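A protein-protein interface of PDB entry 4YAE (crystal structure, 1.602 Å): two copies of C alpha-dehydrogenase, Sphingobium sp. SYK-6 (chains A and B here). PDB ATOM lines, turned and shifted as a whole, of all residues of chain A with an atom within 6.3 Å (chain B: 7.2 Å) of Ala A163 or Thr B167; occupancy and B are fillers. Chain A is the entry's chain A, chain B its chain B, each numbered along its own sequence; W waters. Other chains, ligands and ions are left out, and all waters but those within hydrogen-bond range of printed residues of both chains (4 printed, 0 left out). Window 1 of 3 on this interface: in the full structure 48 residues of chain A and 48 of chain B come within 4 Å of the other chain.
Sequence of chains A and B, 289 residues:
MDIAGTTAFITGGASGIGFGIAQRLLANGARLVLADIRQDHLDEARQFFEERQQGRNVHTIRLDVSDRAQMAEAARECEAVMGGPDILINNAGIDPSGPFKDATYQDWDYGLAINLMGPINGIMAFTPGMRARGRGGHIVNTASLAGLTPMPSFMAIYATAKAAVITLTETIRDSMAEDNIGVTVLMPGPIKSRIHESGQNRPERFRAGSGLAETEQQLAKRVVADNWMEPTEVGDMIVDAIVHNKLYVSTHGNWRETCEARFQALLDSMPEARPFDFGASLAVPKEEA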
ATOM      1  N   ALA A 143     -19.883  25.933 -26.945  1.00  0.00           N
ATOM      2  CA  ALA A 143     -20.527  24.640 -26.949  1.00  0.00           C
ATOM      3  C   ALA A 143     -21.495  24.627 -28.134  1.00  0.00           C
ATOM      4  O   ALA A 143     -21.104  24.952 -29.256  1.00  0.00           O
ATOM      5  CB  ALA A 143     -21.240  24.381 -25.626  1.00  0.00           C
ATOM      6  N   SER A 144     -22.748  24.268 -27.877  1.00  0.00           N
ATOM      7  CA  SER A 144     -23.764  24.184 -28.914  1.00  0.00           C
ATOM      8  C   SER A 144     -25.094  23.937 -28.256  1.00  0.00           C
ATOM      9  O   SER A 144     -25.152  23.345 -27.180  1.00  0.00           O
ATOM     10  CB  SER A 144     -23.459  23.053 -29.896  1.00  0.00           C
ATOM     11  OG  SER A 144     -24.511  22.896 -30.835  1.00  0.00           O
ATOM     12  N   ALA A 146     -26.757  21.822 -29.451  1.00  0.00           N
ATOM     13  CA  ALA A 146     -26.735  20.362 -29.598  1.00  0.00           C
ATOM     14  C   ALA A 146     -26.269  19.671 -28.320  1.00  0.00           C
ATOM     15  O   ALA A 146     -26.425  18.455 -28.167  1.00  0.00           O
ATOM     16  CB  ALA A 146     -25.845  19.957 -30.756  1.00  0.00           C
ATOM     17  N   GLY A 147     -25.694  20.441 -27.403  1.00  0.00           N
ATOM     18  CA  GLY A 147     -25.292  19.909 -26.111  1.00  0.00           C
ATOM     19  C   GLY A 147     -26.405  19.960 -25.083  1.00  0.00           C
ATOM     20  O   GLY A 147     -26.219  19.510 -23.948  1.00  0.00           O
ATOM     21  N   LEU A 148     -27.568  20.482 -25.479  1.00  0.00           N
ATOM     22  CA  LEU A 148     -28.662  20.738 -24.544  1.00  0.00           C
ATOM     23  C   LEU A 148     -29.995  20.133 -24.991  1.00  0.00           C
ATOM     24  O   LEU A 148     -30.696  19.504 -24.195  1.00  0.00           O
ATOM     25  CB  LEU A 148     -28.807  22.255 -24.348  1.00  0.00           C
ATOM     26  CG  LEU A 148     -29.342  22.767 -23.020  1.00  0.00           C
ATOM     27  CD1 LEU A 148     -28.501  22.274 -21.857  1.00  0.00           C
ATOM     28  CD2 LEU A 148     -29.366  24.287 -23.054  1.00  0.00           C
ATOM     29  N   ALA A 156     -24.224  11.894 -32.161  1.00  0.00           N
ATOM     30  CA  ALA A 156     -23.842  11.479 -30.810  1.00  0.00           C
ATOM     31  C   ALA A 156     -22.496  12.044 -30.339  1.00  0.00           C
ATOM     32  O   ALA A 156     -22.378  12.508 -29.211  1.00  0.00           O
ATOM     33  CB  ALA A 156     -23.816   9.964 -30.735  1.00  0.00           C
ATOM     34  N   TYR A 158     -20.658  14.679 -31.384  1.00  0.00           N
ATOM     35  CA  TYR A 158     -20.694  16.124 -31.252  1.00  0.00           C
ATOM     36  C   TYR A 158     -21.527  16.533 -30.041  1.00  0.00           C
ATOM     37  O   TYR A 158     -21.097  17.357 -29.237  1.00  0.00           O
ATOM     38  CB  TYR A 158     -21.258  16.753 -32.523  1.00  0.00           C
ATOM     39  CG  TYR A 158     -21.189  18.262 -32.569  1.00  0.00           C
ATOM     40  CD1 TYR A 158     -20.001  18.921 -32.883  1.00  0.00           C
ATOM     41  CD2 TYR A 158     -22.312  19.028 -32.315  1.00  0.00           C
ATOM     42  CE1 TYR A 158     -19.943  20.302 -32.939  1.00  0.00           C
ATOM     43  CE2 TYR A 158     -22.267  20.416 -32.376  1.00  0.00           C
ATOM     44  CZ  TYR A 158     -21.081  21.044 -32.684  1.00  0.00           C
ATOM     45  OH  TYR A 158     -21.034  22.420 -32.734  1.00  0.00           O
ATOM     46  N   ALA A 159     -22.714  15.954 -29.906  1.00  0.00           N
ATOM     47  CA  ALA A 159     -23.587  16.326 -28.801  1.00  0.00           C
ATOM     48  C   ALA A 159     -22.949  16.015 -27.450  1.00  0.00           C
ATOM     49  O   ALA A 159     -23.044  16.812 -26.510  1.00  0.00           O
ATOM     50  CB  ALA A 159     -24.919  15.620 -28.910  1.00  0.00           C
ATOM     51  N   THR A 160     -22.332  14.840 -27.356  1.00  0.00           N
ATOM     52  CA  THR A 160     -21.694  14.382 -26.130  1.00  0.00           C
ATOM     53  C   THR A 160     -20.583  15.351 -25.716  1.00  0.00           C
ATOM     54  O   THR A 160     -20.509  15.765 -24.558  1.00  0.00           O
ATOM     55  CB  THR A 160     -21.134  12.952 -26.306  1.00  0.00           C
ATOM     56  OG1 THR A 160     -22.217  12.042 -26.539  1.00  0.00           O
ATOM     57  CG2 THR A 160     -20.379  12.485 -25.084  1.00  0.00           C
ATOM     58  N   ALA A 161     -19.739  15.733 -26.667  1.00  0.00           N
ATOM     59  CA  ALA A 161     -18.650  16.657 -26.370  1.00  0.00           C
ATOM     60  C   ALA A 161     -19.161  18.023 -25.929  1.00  0.00           C
ATOM     61  O   ALA A 161     -18.632  18.625 -24.983  1.00  0.00           O
ATOM     62  CB  ALA A 161     -17.737  16.816 -27.584  1.00  0.00           C
ATOM     63  N   LYS A 162     -20.172  18.534 -26.623  1.00  0.00           N
ATOM     64  CA  LYS A 162     -20.637  19.892 -26.356  1.00  0.00           C
ATOM     65  C   LYS A 162     -21.417  19.971 -25.049  1.00  0.00           C
ATOM     66  O   LYS A 162     -21.370  20.989 -24.366  1.00  0.00           O
ATOM     67  CB  LYS A 162     -21.472  20.408 -27.527  1.00  0.00           C
ATOM     68  CG  LYS A 162     -20.677  20.560 -28.820  1.00  0.00           C
ATOM     69  CD  LYS A 162     -19.493  21.480 -28.652  1.00  0.00           C
ATOM     70  CE  LYS A 162     -18.819  21.775 -29.979  1.00  0.00           C
ATOM     71  NZ  LYS A 162     -17.952  22.960 -29.843  1.00  0.00           N
ATOM     72  N   ALA A 163     -22.131  18.903 -24.694  1.00  0.00           N
ATOM     73  CA  ALA A 163     -22.775  18.831 -23.379  1.00  0.00           C
ATOM     74  C   ALA A 163     -21.725  18.938 -22.274  1.00  0.00           C
ATOM     75  O   ALA A 163     -21.916  19.634 -21.271  1.00  0.00           O
ATOM     76  CB  ALA A 163     -23.567  17.539 -23.241  1.00  0.00           C
ATOM     77  N   ALA A 164     -20.613  18.242 -22.465  1.00  0.00           N
ATOM     78  CA  ALA A 164     -19.500  18.297 -21.525  1.00  0.00           C
ATOM     79  C   ALA A 164     -18.969  19.729 -21.369  1.00  0.00           C
ATOM     80  O   ALA A 164     -18.654  20.170 -20.260  1.00  0.00           O
ATOM     81  CB  ALA A 164     -18.390  17.373 -21.976  1.00  0.00           C
ATOM     82  N   VAL A 165     -18.861  20.445 -22.482  1.00  0.00           N
ATOM     83  CA  VAL A 165     -18.337  21.805 -22.453  1.00  0.00           C
ATOM     84  C   VAL A 165     -19.249  22.734 -21.642  1.00  0.00           C
ATOM     85  O   VAL A 165     -18.760  23.626 -20.944  1.00  0.00           O
ATOM     86  CB  VAL A 165     -18.150  22.362 -23.883  1.00  0.00           C
ATOM     87  CG1 VAL A 165     -17.755  23.849 -23.869  1.00  0.00           C
ATOM     88  CG2 VAL A 165     -17.101  21.562 -24.617  1.00  0.00           C
ATOM     89  N   ILE A 166     -20.563  22.540 -21.738  1.00  0.00           N
ATOM     90  CA  ILE A 166     -21.502  23.350 -20.960  1.00  0.00           C
ATOM     91  C   ILE A 166     -21.236  23.148 -19.470  1.00  0.00           C
ATOM     92  O   ILE A 166     -21.068  24.104 -18.720  1.00  0.00           O
ATOM     93  CB  ILE A 166     -22.960  23.007 -21.288  1.00  0.00           C
ATOM     94  CG1 ILE A 166     -23.285  23.415 -22.726  1.00  0.00           C
ATOM     95  CG2 ILE A 166     -23.927  23.733 -20.333  1.00  0.00           C
ATOM     96  CD1 ILE A 166     -24.626  22.903 -23.237  1.00  0.00           C
ATOM     97  N   THR A 167     -21.172  21.893 -19.046  1.00  0.00           N
ATOM     98  CA  THR A 167     -20.974  21.580 -17.638  1.00  0.00           C
ATOM     99  C   THR A 167     -19.588  22.003 -17.146  1.00  0.00           C
ATOM    100  O   THR A 167     -19.437  22.490 -16.032  1.00  0.00           O
ATOM    101  CB  THR A 167     -21.184  20.089 -17.406  1.00  0.00           C
ATOM    102  OG1 THR A 167     -22.545  19.772 -17.714  1.00  0.00           O
ATOM    103  CG2 THR A 167     -20.878  19.696 -15.962  1.00  0.00           C
ATOM    104  N   LEU A 168     -18.583  21.821 -17.993  1.00  0.00           N
ATOM    105  CA  LEU A 168     -17.226  22.279 -17.689  1.00  0.00           C
ATOM    106  C   LEU A 168     -17.241  23.755 -17.321  1.00  0.00           C
ATOM    107  O   LEU A 168     -16.672  24.162 -16.311  1.00  0.00           O
ATOM    108  CB  LEU A 168     -16.306  22.036 -18.884  1.00  0.00           C
ATOM    109  CG  LEU A 168     -14.950  22.756 -18.900  1.00  0.00           C
ATOM    110  CD1 LEU A 168     -14.059  22.198 -17.818  1.00  0.00           C
ATOM    111  CD2 LEU A 168     -14.305  22.623 -20.272  1.00  0.00           C
ATOM    112  N   ARG A 262     -37.250  18.109 -22.551  1.00  0.00           N
ATOM    113  CA  ARG A 262     -36.174  17.276 -22.022  1.00  0.00           C
ATOM    114  C   ARG A 262     -35.996  17.525 -20.529  1.00  0.00           C
ATOM    115  O   ARG A 262     -35.899  16.588 -19.739  1.00  0.00           O
ATOM    116  CB  ARG A 262     -34.849  17.541 -22.753  1.00  0.00           C
ATOM    117  CG  ARG A 262     -33.680  16.740 -22.175  1.00  0.00           C
ATOM    118  CD  ARG A 262     -32.320  17.121 -22.767  1.00  0.00           C
ATOM    119  NE  ARG A 262     -31.257  16.438 -22.020  1.00  0.00           N
ATOM    120  CZ  ARG A 262     -30.168  17.009 -21.514  1.00  0.00           C
ATOM    121  NH1 ARG A 262     -29.904  18.295 -21.707  1.00  0.00           N
ATOM    122  NH2 ARG A 262     -29.304  16.266 -20.834  1.00  0.00           N
ATOM    123  N   ALA B 143     -24.238   7.538 -14.844  1.00  0.00           N
ATOM    124  CA  ALA B 143     -23.769   8.910 -14.798  1.00  0.00           C
ATOM    125  C   ALA B 143     -23.826   9.367 -13.340  1.00  0.00           C
ATOM    126  O   ALA B 143     -23.298   8.684 -12.464  1.00  0.00           O
ATOM    127  CB  ALA B 143     -24.599   9.804 -15.707  1.00  0.00           C
ATOM    128  N   GLY B 147     -23.862  15.334 -12.872  1.00  0.00           N
ATOM    129  CA  GLY B 147     -23.830  15.704 -14.278  1.00  0.00           C
ATOM    130  C   GLY B 147     -24.986  16.603 -14.668  1.00  0.00           C
ATOM    131  O   GLY B 147     -25.083  17.020 -15.821  1.00  0.00           O
ATOM    132  N   ALA B 159     -18.011  16.070 -12.799  1.00  0.00           N
ATOM    133  CA  ALA B 159     -19.261  16.638 -13.312  1.00  0.00           C
ATOM    134  C   ALA B 159     -19.267  16.669 -14.841  1.00  0.00           C
ATOM    135  O   ALA B 159     -20.257  16.317 -15.479  1.00  0.00           O
ATOM    136  CB  ALA B 159     -19.470  18.017 -12.766  1.00  0.00           C
ATOM    137  N   THR B 160     -18.149  17.093 -15.418  1.00  0.00           N
ATOM    138  CA  THR B 160     -18.001  17.195 -16.860  1.00  0.00           C
ATOM    139  C   THR B 160     -18.164  15.832 -17.540  1.00  0.00           C
ATOM    140  O   THR B 160     -18.924  15.682 -18.501  1.00  0.00           O
ATOM    141  CB  THR B 160     -16.621  17.805 -17.211  1.00  0.00           C
ATOM    142  OG1 THR B 160     -16.564  19.156 -16.735  1.00  0.00           O
ATOM    143  CG2 THR B 160     -16.372  17.814 -18.712  1.00  0.00           C
ATOM    144  N   LYS B 162     -19.588  13.112 -16.296  1.00  0.00           N
ATOM    145  CA  LYS B 162     -20.902  12.521 -16.070  1.00  0.00           C
ATOM    146  C   LYS B 162     -21.991  13.204 -16.898  1.00  0.00           C
ATOM    147  O   LYS B 162     -22.912  12.534 -17.368  1.00  0.00           O
ATOM    148  CB  LYS B 162     -21.255  12.557 -14.583  1.00  0.00           C
ATOM    149  CG  LYS B 162     -20.336  11.686 -13.710  1.00  0.00           C
ATOM    150  CD  LYS B 162     -20.300  10.254 -14.179  1.00  0.00           C
ATOM    151  CE  LYS B 162     -19.661   9.325 -13.152  1.00  0.00           C
ATOM    152  NZ  LYS B 162     -19.895   7.903 -13.494  1.00  0.00           N
ATOM    153  N   ALA B 163     -21.889  14.520 -17.088  1.00  0.00           N
ATOM    154  CA  ALA B 163     -22.801  15.225 -17.979  1.00  0.00           C
ATOM    155  C   ALA B 163     -22.722  14.639 -19.383  1.00  0.00           C
ATOM    156  O   ALA B 163     -23.740  14.447 -20.046  1.00  0.00           O
ATOM    157  CB  ALA B 163     -22.490  16.707 -18.007  1.00  0.00           C
ATOM    158  N   ALA B 164     -21.508  14.338 -19.829  1.00  0.00           N
ATOM    159  CA  ALA B 164     -21.320  13.774 -21.161  1.00  0.00           C
ATOM    160  C   ALA B 164     -21.997  12.405 -21.281  1.00  0.00           C
ATOM    161  O   ALA B 164     -22.568  12.086 -22.321  1.00  0.00           O
ATOM    162  CB  ALA B 164     -19.857  13.659 -21.484  1.00  0.00           C
ATOM    163  N   VAL B 165     -21.942  11.601 -20.223  1.00  0.00           N
ATOM    164  CA  VAL B 165     -22.560  10.275 -20.255  1.00  0.00           C
ATOM    165  C   VAL B 165     -24.087  10.376 -20.376  1.00  0.00           C
ATOM    166  O   VAL B 165     -24.715   9.550 -21.033  1.00  0.00           O
ATOM    167  CB  VAL B 165     -22.167   9.443 -19.002  1.00  0.00           C
ATOM    168  CG1 VAL B 165     -22.949   8.128 -18.935  1.00  0.00           C
ATOM    169  CG2 VAL B 165     -20.686   9.178 -19.022  1.00  0.00           C
ATOM    170  N   ILE B 166     -24.688  11.390 -19.763  1.00  0.00           N
ATOM    171  CA  ILE B 166     -26.131  11.580 -19.886  1.00  0.00           C
ATOM    172  C   ILE B 166     -26.478  11.820 -21.360  1.00  0.00           C
ATOM    173  O   ILE B 166     -27.339  11.150 -21.921  1.00  0.00           O
ATOM    174  CB  ILE B 166     -26.638  12.752 -18.994  1.00  0.00           C
ATOM    175  CG1 ILE B 166     -26.440  12.404 -17.513  1.00  0.00           C
ATOM    176  CG2 ILE B 166     -28.105  13.028 -19.262  1.00  0.00           C
ATOM    177  CD1 ILE B 166     -26.626  13.594 -16.573  1.00  0.00           C
ATOM    178  N   THR B 167     -25.770  12.741 -22.003  1.00  0.00           N
ATOM    179  CA  THR B 167     -26.034  13.056 -23.396  1.00  0.00           C
ATOM    180  C   THR B 167     -25.687  11.899 -24.337  1.00  0.00           C
ATOM    181  O   THR B 167     -26.424  11.630 -25.288  1.00  0.00           O
ATOM    182  CB  THR B 167     -25.266  14.322 -23.779  1.00  0.00           C
ATOM    183  OG1 THR B 167     -25.749  15.393 -22.956  1.00  0.00           O
ATOM    184  CG2 THR B 167     -25.442  14.666 -25.250  1.00  0.00           C
ATOM    185  N   LEU B 168     -24.580  11.214 -24.065  1.00  0.00           N
ATOM    186  CA  LEU B 168     -24.222  10.008 -24.806  1.00  0.00           C
ATOM    187  C   LEU B 168     -25.405   9.047 -24.852  1.00  0.00           C
ATOM    188  O   LEU B 168     -25.791   8.558 -25.911  1.00  0.00           O
ATOM    189  CB  LEU B 168     -23.022   9.324 -24.163  1.00  0.00           C
ATOM    190  CG  LEU B 168     -22.686   7.906 -24.645  1.00  0.00           C
ATOM    191  CD1 LEU B 168     -22.183   7.931 -26.082  1.00  0.00           C
ATOM    192  CD2 LEU B 168     -21.660   7.282 -23.721  1.00  0.00           C
ATOM    193  N   THR B 169     -25.979   8.781 -23.684  1.00  0.00           N
ATOM    194  CA  THR B 169     -27.042   7.787 -23.572  1.00  0.00           C
ATOM    195  C   THR B 169     -28.294   8.232 -24.323  1.00  0.00           C
ATOM    196  O   THR B 169     -28.889   7.455 -25.069  1.00  0.00           O
ATOM    197  CB  THR B 169     -27.392   7.516 -22.096  1.00  0.00           C
ATOM    198  OG1 THR B 169     -26.193   7.239 -21.368  1.00  0.00           O
ATOM    199  CG2 THR B 169     -28.332   6.317 -21.969  1.00  0.00           C
ATOM    200  N   GLU B 170     -28.698   9.483 -24.123  1.00  0.00           N
ATOM    201  CA  GLU B 170     -29.815  10.045 -24.871  1.00  0.00           C
ATOM    202  C   GLU B 170     -29.627   9.904 -26.374  1.00  0.00           C
ATOM    203  O   GLU B 170     -30.535   9.497 -27.090  1.00  0.00           O
ATOM    204  CB  GLU B 170     -29.996  11.526 -24.527  1.00  0.00           C
ATOM    205  CG  GLU B 170     -30.340  11.807 -23.077  1.00  0.00           C
ATOM    206  CD  GLU B 170     -30.286  13.298 -22.751  1.00  0.00           C
ATOM    207  OE1 GLU B 170     -29.620  14.052 -23.502  1.00  0.00           O
ATOM    208  OE2 GLU B 170     -30.932  13.728 -21.768  1.00  0.00           O
ATOM    209  N   THR B 171     -28.445  10.244 -26.869  1.00  0.00           N
ATOM    210  CA  THR B 171     -28.280  10.345 -28.308  1.00  0.00           C
ATOM    211  C   THR B 171     -28.202   8.990 -28.989  1.00  0.00           C
ATOM    212  O   THR B 171     -28.666   8.853 -30.126  1.00  0.00           O
ATOM    213  CB  THR B 171     -27.036  11.173 -28.674  1.00  0.00           C
ATOM    214  OG1 THR B 171     -25.852  10.513 -28.194  1.00  0.00           O
ATOM    215  CG2 THR B 171     -27.168  12.559 -28.069  1.00  0.00           C
ATOM    216  N   ILE B 172     -27.653   7.981 -28.319  1.00  0.00           N
ATOM    217  CA  ILE B 172     -27.522   6.676 -28.961  1.00  0.00           C
ATOM    218  C   ILE B 172     -28.828   5.885 -28.966  1.00  0.00           C
ATOM    219  O   ILE B 172     -28.901   4.835 -29.604  1.00  0.00           O
ATOM    220  CB  ILE B 172     -26.447   5.796 -28.298  1.00  0.00           C
ATOM    221  CG1 ILE B 172     -26.828   5.442 -26.855  1.00  0.00           C
ATOM    222  CG2 ILE B 172     -25.065   6.477 -28.384  1.00  0.00           C
ATOM    223  CD1 ILE B 172     -25.795   4.529 -26.142  1.00  0.00           C
ATOM    224  N   ARG B 173     -29.836   6.363 -28.248  1.00  0.00           N
ATOM    225  CA  ARG B 173     -31.081   5.595 -28.093  1.00  0.00           C
ATOM    226  C   ARG B 173     -31.654   5.129 -29.430  1.00  0.00           C
ATOM    227  O   ARG B 173     -32.019   3.961 -29.578  1.00  0.00           O
ATOM    228  CB  ARG B 173     -32.138   6.417 -27.348  1.00  0.00           C
ATOM    229  CG  ARG B 173     -33.348   5.584 -26.927  1.00  0.00           C
ATOM    230  CD  ARG B 173     -34.414   6.412 -26.254  1.00  0.00           C
ATOM    231  NE  ARG B 173     -35.189   5.602 -25.325  1.00  0.00           N
ATOM    232  CZ  ARG B 173     -36.269   6.029 -24.685  1.00  0.00           C
ATOM    233  NH1 ARG B 173     -36.735   7.265 -24.897  1.00  0.00           N
ATOM    234  NH2 ARG B 173     -36.876   5.217 -23.834  1.00  0.00           N
ATOM    235  N   VAL B 185     -29.871   5.836 -18.694  1.00  0.00           N
ATOM    236  CA  VAL B 185     -28.814   6.470 -17.924  1.00  0.00           C
ATOM    237  C   VAL B 185     -29.282   6.585 -16.473  1.00  0.00           C
ATOM    238  O   VAL B 185     -30.372   7.101 -16.160  1.00  0.00           O
ATOM    239  CB  VAL B 185     -28.388   7.835 -18.503  1.00  0.00           C
ATOM    240  CG1 VAL B 185     -29.543   8.789 -18.597  1.00  0.00           C
ATOM    241  CG2 VAL B 185     -27.249   8.428 -17.661  1.00  0.00           C
ATOM    242  N   ARG B 262     -31.203  25.761 -12.507  1.00  0.00           N
ATOM    243  CA  ARG B 262     -30.254  25.723 -13.608  1.00  0.00           C
ATOM    244  C   ARG B 262     -30.982  25.700 -14.946  1.00  0.00           C
ATOM    245  O   ARG B 262     -30.631  26.439 -15.868  1.00  0.00           O
ATOM    246  CB  ARG B 262     -29.342  24.497 -13.496  1.00  0.00           C
ATOM    247  CG  ARG B 262     -28.311  24.409 -14.613  1.00  0.00           C
ATOM    248  CD  ARG B 262     -27.640  23.053 -14.694  1.00  0.00           C
ATOM    249  NE  ARG B 262     -26.870  22.957 -15.934  1.00  0.00           N
ATOM    250  CZ  ARG B 262     -26.805  21.886 -16.712  1.00  0.00           C
ATOM    251  NH1 ARG B 262     -27.426  20.762 -16.380  1.00  0.00           N
ATOM    252  NH2 ARG B 262     -26.076  21.931 -17.828  1.00  0.00           N
HETATM  253  O   HOH W   1     -24.676  19.909 -19.547  1.00  0.00           O
HETATM  254  O   HOH W   2     -26.274  16.440 -20.309  1.00  0.00           O
HETATM  255  O   HOH W   3     -24.162  20.537 -15.735  1.00  0.00           O
HETATM  256  O   HOH W   4     -28.157  16.390 -23.837  1.00  0.00           O
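Ala A159 touches Thr B167, and with the chains exchanged Thr A167 touches Ala B159. Thr A160 touches Ala B164, and with the chains exchanged Ala A164 touches Thr B160. Thr A160 touches Leu B168, and with the chains exchanged Leu A168 touches Thr B160. Ile A166 touches Arg B262, and with the chains exchanged Arg A262 touches Ile B166. 12 positions are printed for both chains. Of the 15 pairs that touch across the chains among the printed residues, 12 have their exchanged pair printed and touching as well.
OE2 of Glu B170 is in salt-bridge range of NE of Arg A262 (2.7 Å).
Among the printed residues, merely in contact across the chains: Ala A163 with Thr B167 (3.1 Å), Thr A167 with Ala B163 (3.1 Å), Ala A156 with Thr B171 (3.3 Å), Leu A168 with Thr B160 (3.3 Å), Thr A160 with Leu B168 (3.3 Å), Ala A159 with Thr B167 (3.5 Å), Thr A167 with Ala B159 (3.5 Å), Thr A160 with Ala B164 (3.5 Å), Ala A164 with Thr B160 (3.6 Å), Thr A160 with Thr B167 (3.8 Å), Ile A166 with Arg B262 (3.8 Å), Arg A262 with Ile B166 (3.8 Å), Thr A167 with Thr B160 (3.8 Å) and Ala A159 with Thr B171 (3.9 Å).
Water W3 bridges the side-chain hydroxyl (OG1) of Thr A167 and the guanidinium group (NH2) of Arg B262. Water W4 lies within hydrogen-bond range of OG1 of Thr B167 (2.8 Å), OE1 of Glu B170 (2.8 Å) and NH2 of Arg A262 (3.2 Å). Water W1 lies within hydrogen-bond range of the side-chain hydroxyl (OG1) of Thr A167 (2.8 Å), the guanidinium group (NH2) of Arg B262 (3.0 Å) and the backbone carbonyl oxygen (O) of Ala A163 (3.3 Å). Water W2 lies within hydrogen-bond range of OG1 of Thr B167 (2.9 Å), NH2 of Arg A262 (3.1 Å) and O of Ala B163 (3.2 Å).
Of chain B, only Thr B167 comes within 4 Å of Ala A163. Of the printed residues of chain A, Ala B159 touches Thr A167. Of the printed residues of chain A, Thr B160 touches Ala A164 (3.6 Å), Thr A167 (3.8 Å) and Leu A168 (3.3 Å). Of the printed residues of chain A, Glu B170 touches Arg A262 (2.7 Å). Of the printed residues of chain A, Ala B164 touches Thr A160. Ala B143 touches none of the printed residues of chain A. Ser A144 touches none of the printed residues of chain B. The nearest residue of chain B that does not touch Ala A163 is Ala B163 (4.4 Å). The nearest printed residue of chain A that does not touch Ile B166 is Ala A163 (6.7 Å).
OG1 of Thr B171 sits close to O of Thr B167 (3.2 Å). The backbone carbonyl oxygen (O) of Leu A148 lies within hydrogen-bond range of the guanidinium group (NH1) of Arg A262, at 2.9 Å. O of Leu B168 sits at hydrogen-bond distance from OG1 of Thr B171 (3.0 Å). The side-chain hydroxyl (OG1) of Thr A160 lies within hydrogen-bond range of the backbone carbonyl oxygen (O) of Ala A156 (2.7 Å).
Hydrophobic or aromatic side chains of chain B within 4 Å of the printed part of chain A: Ala B159, Ala B163, Ala B164, Ile B166 and Leu B168. Of the 18 printed residues of chain A, 9 touch a printed residue of chain B. Among the printed residues, Asp or Glu carboxylates within 4 Å of a Lys or Arg side-chain nitrogen of the other chain: Arg A262 with Glu B170.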
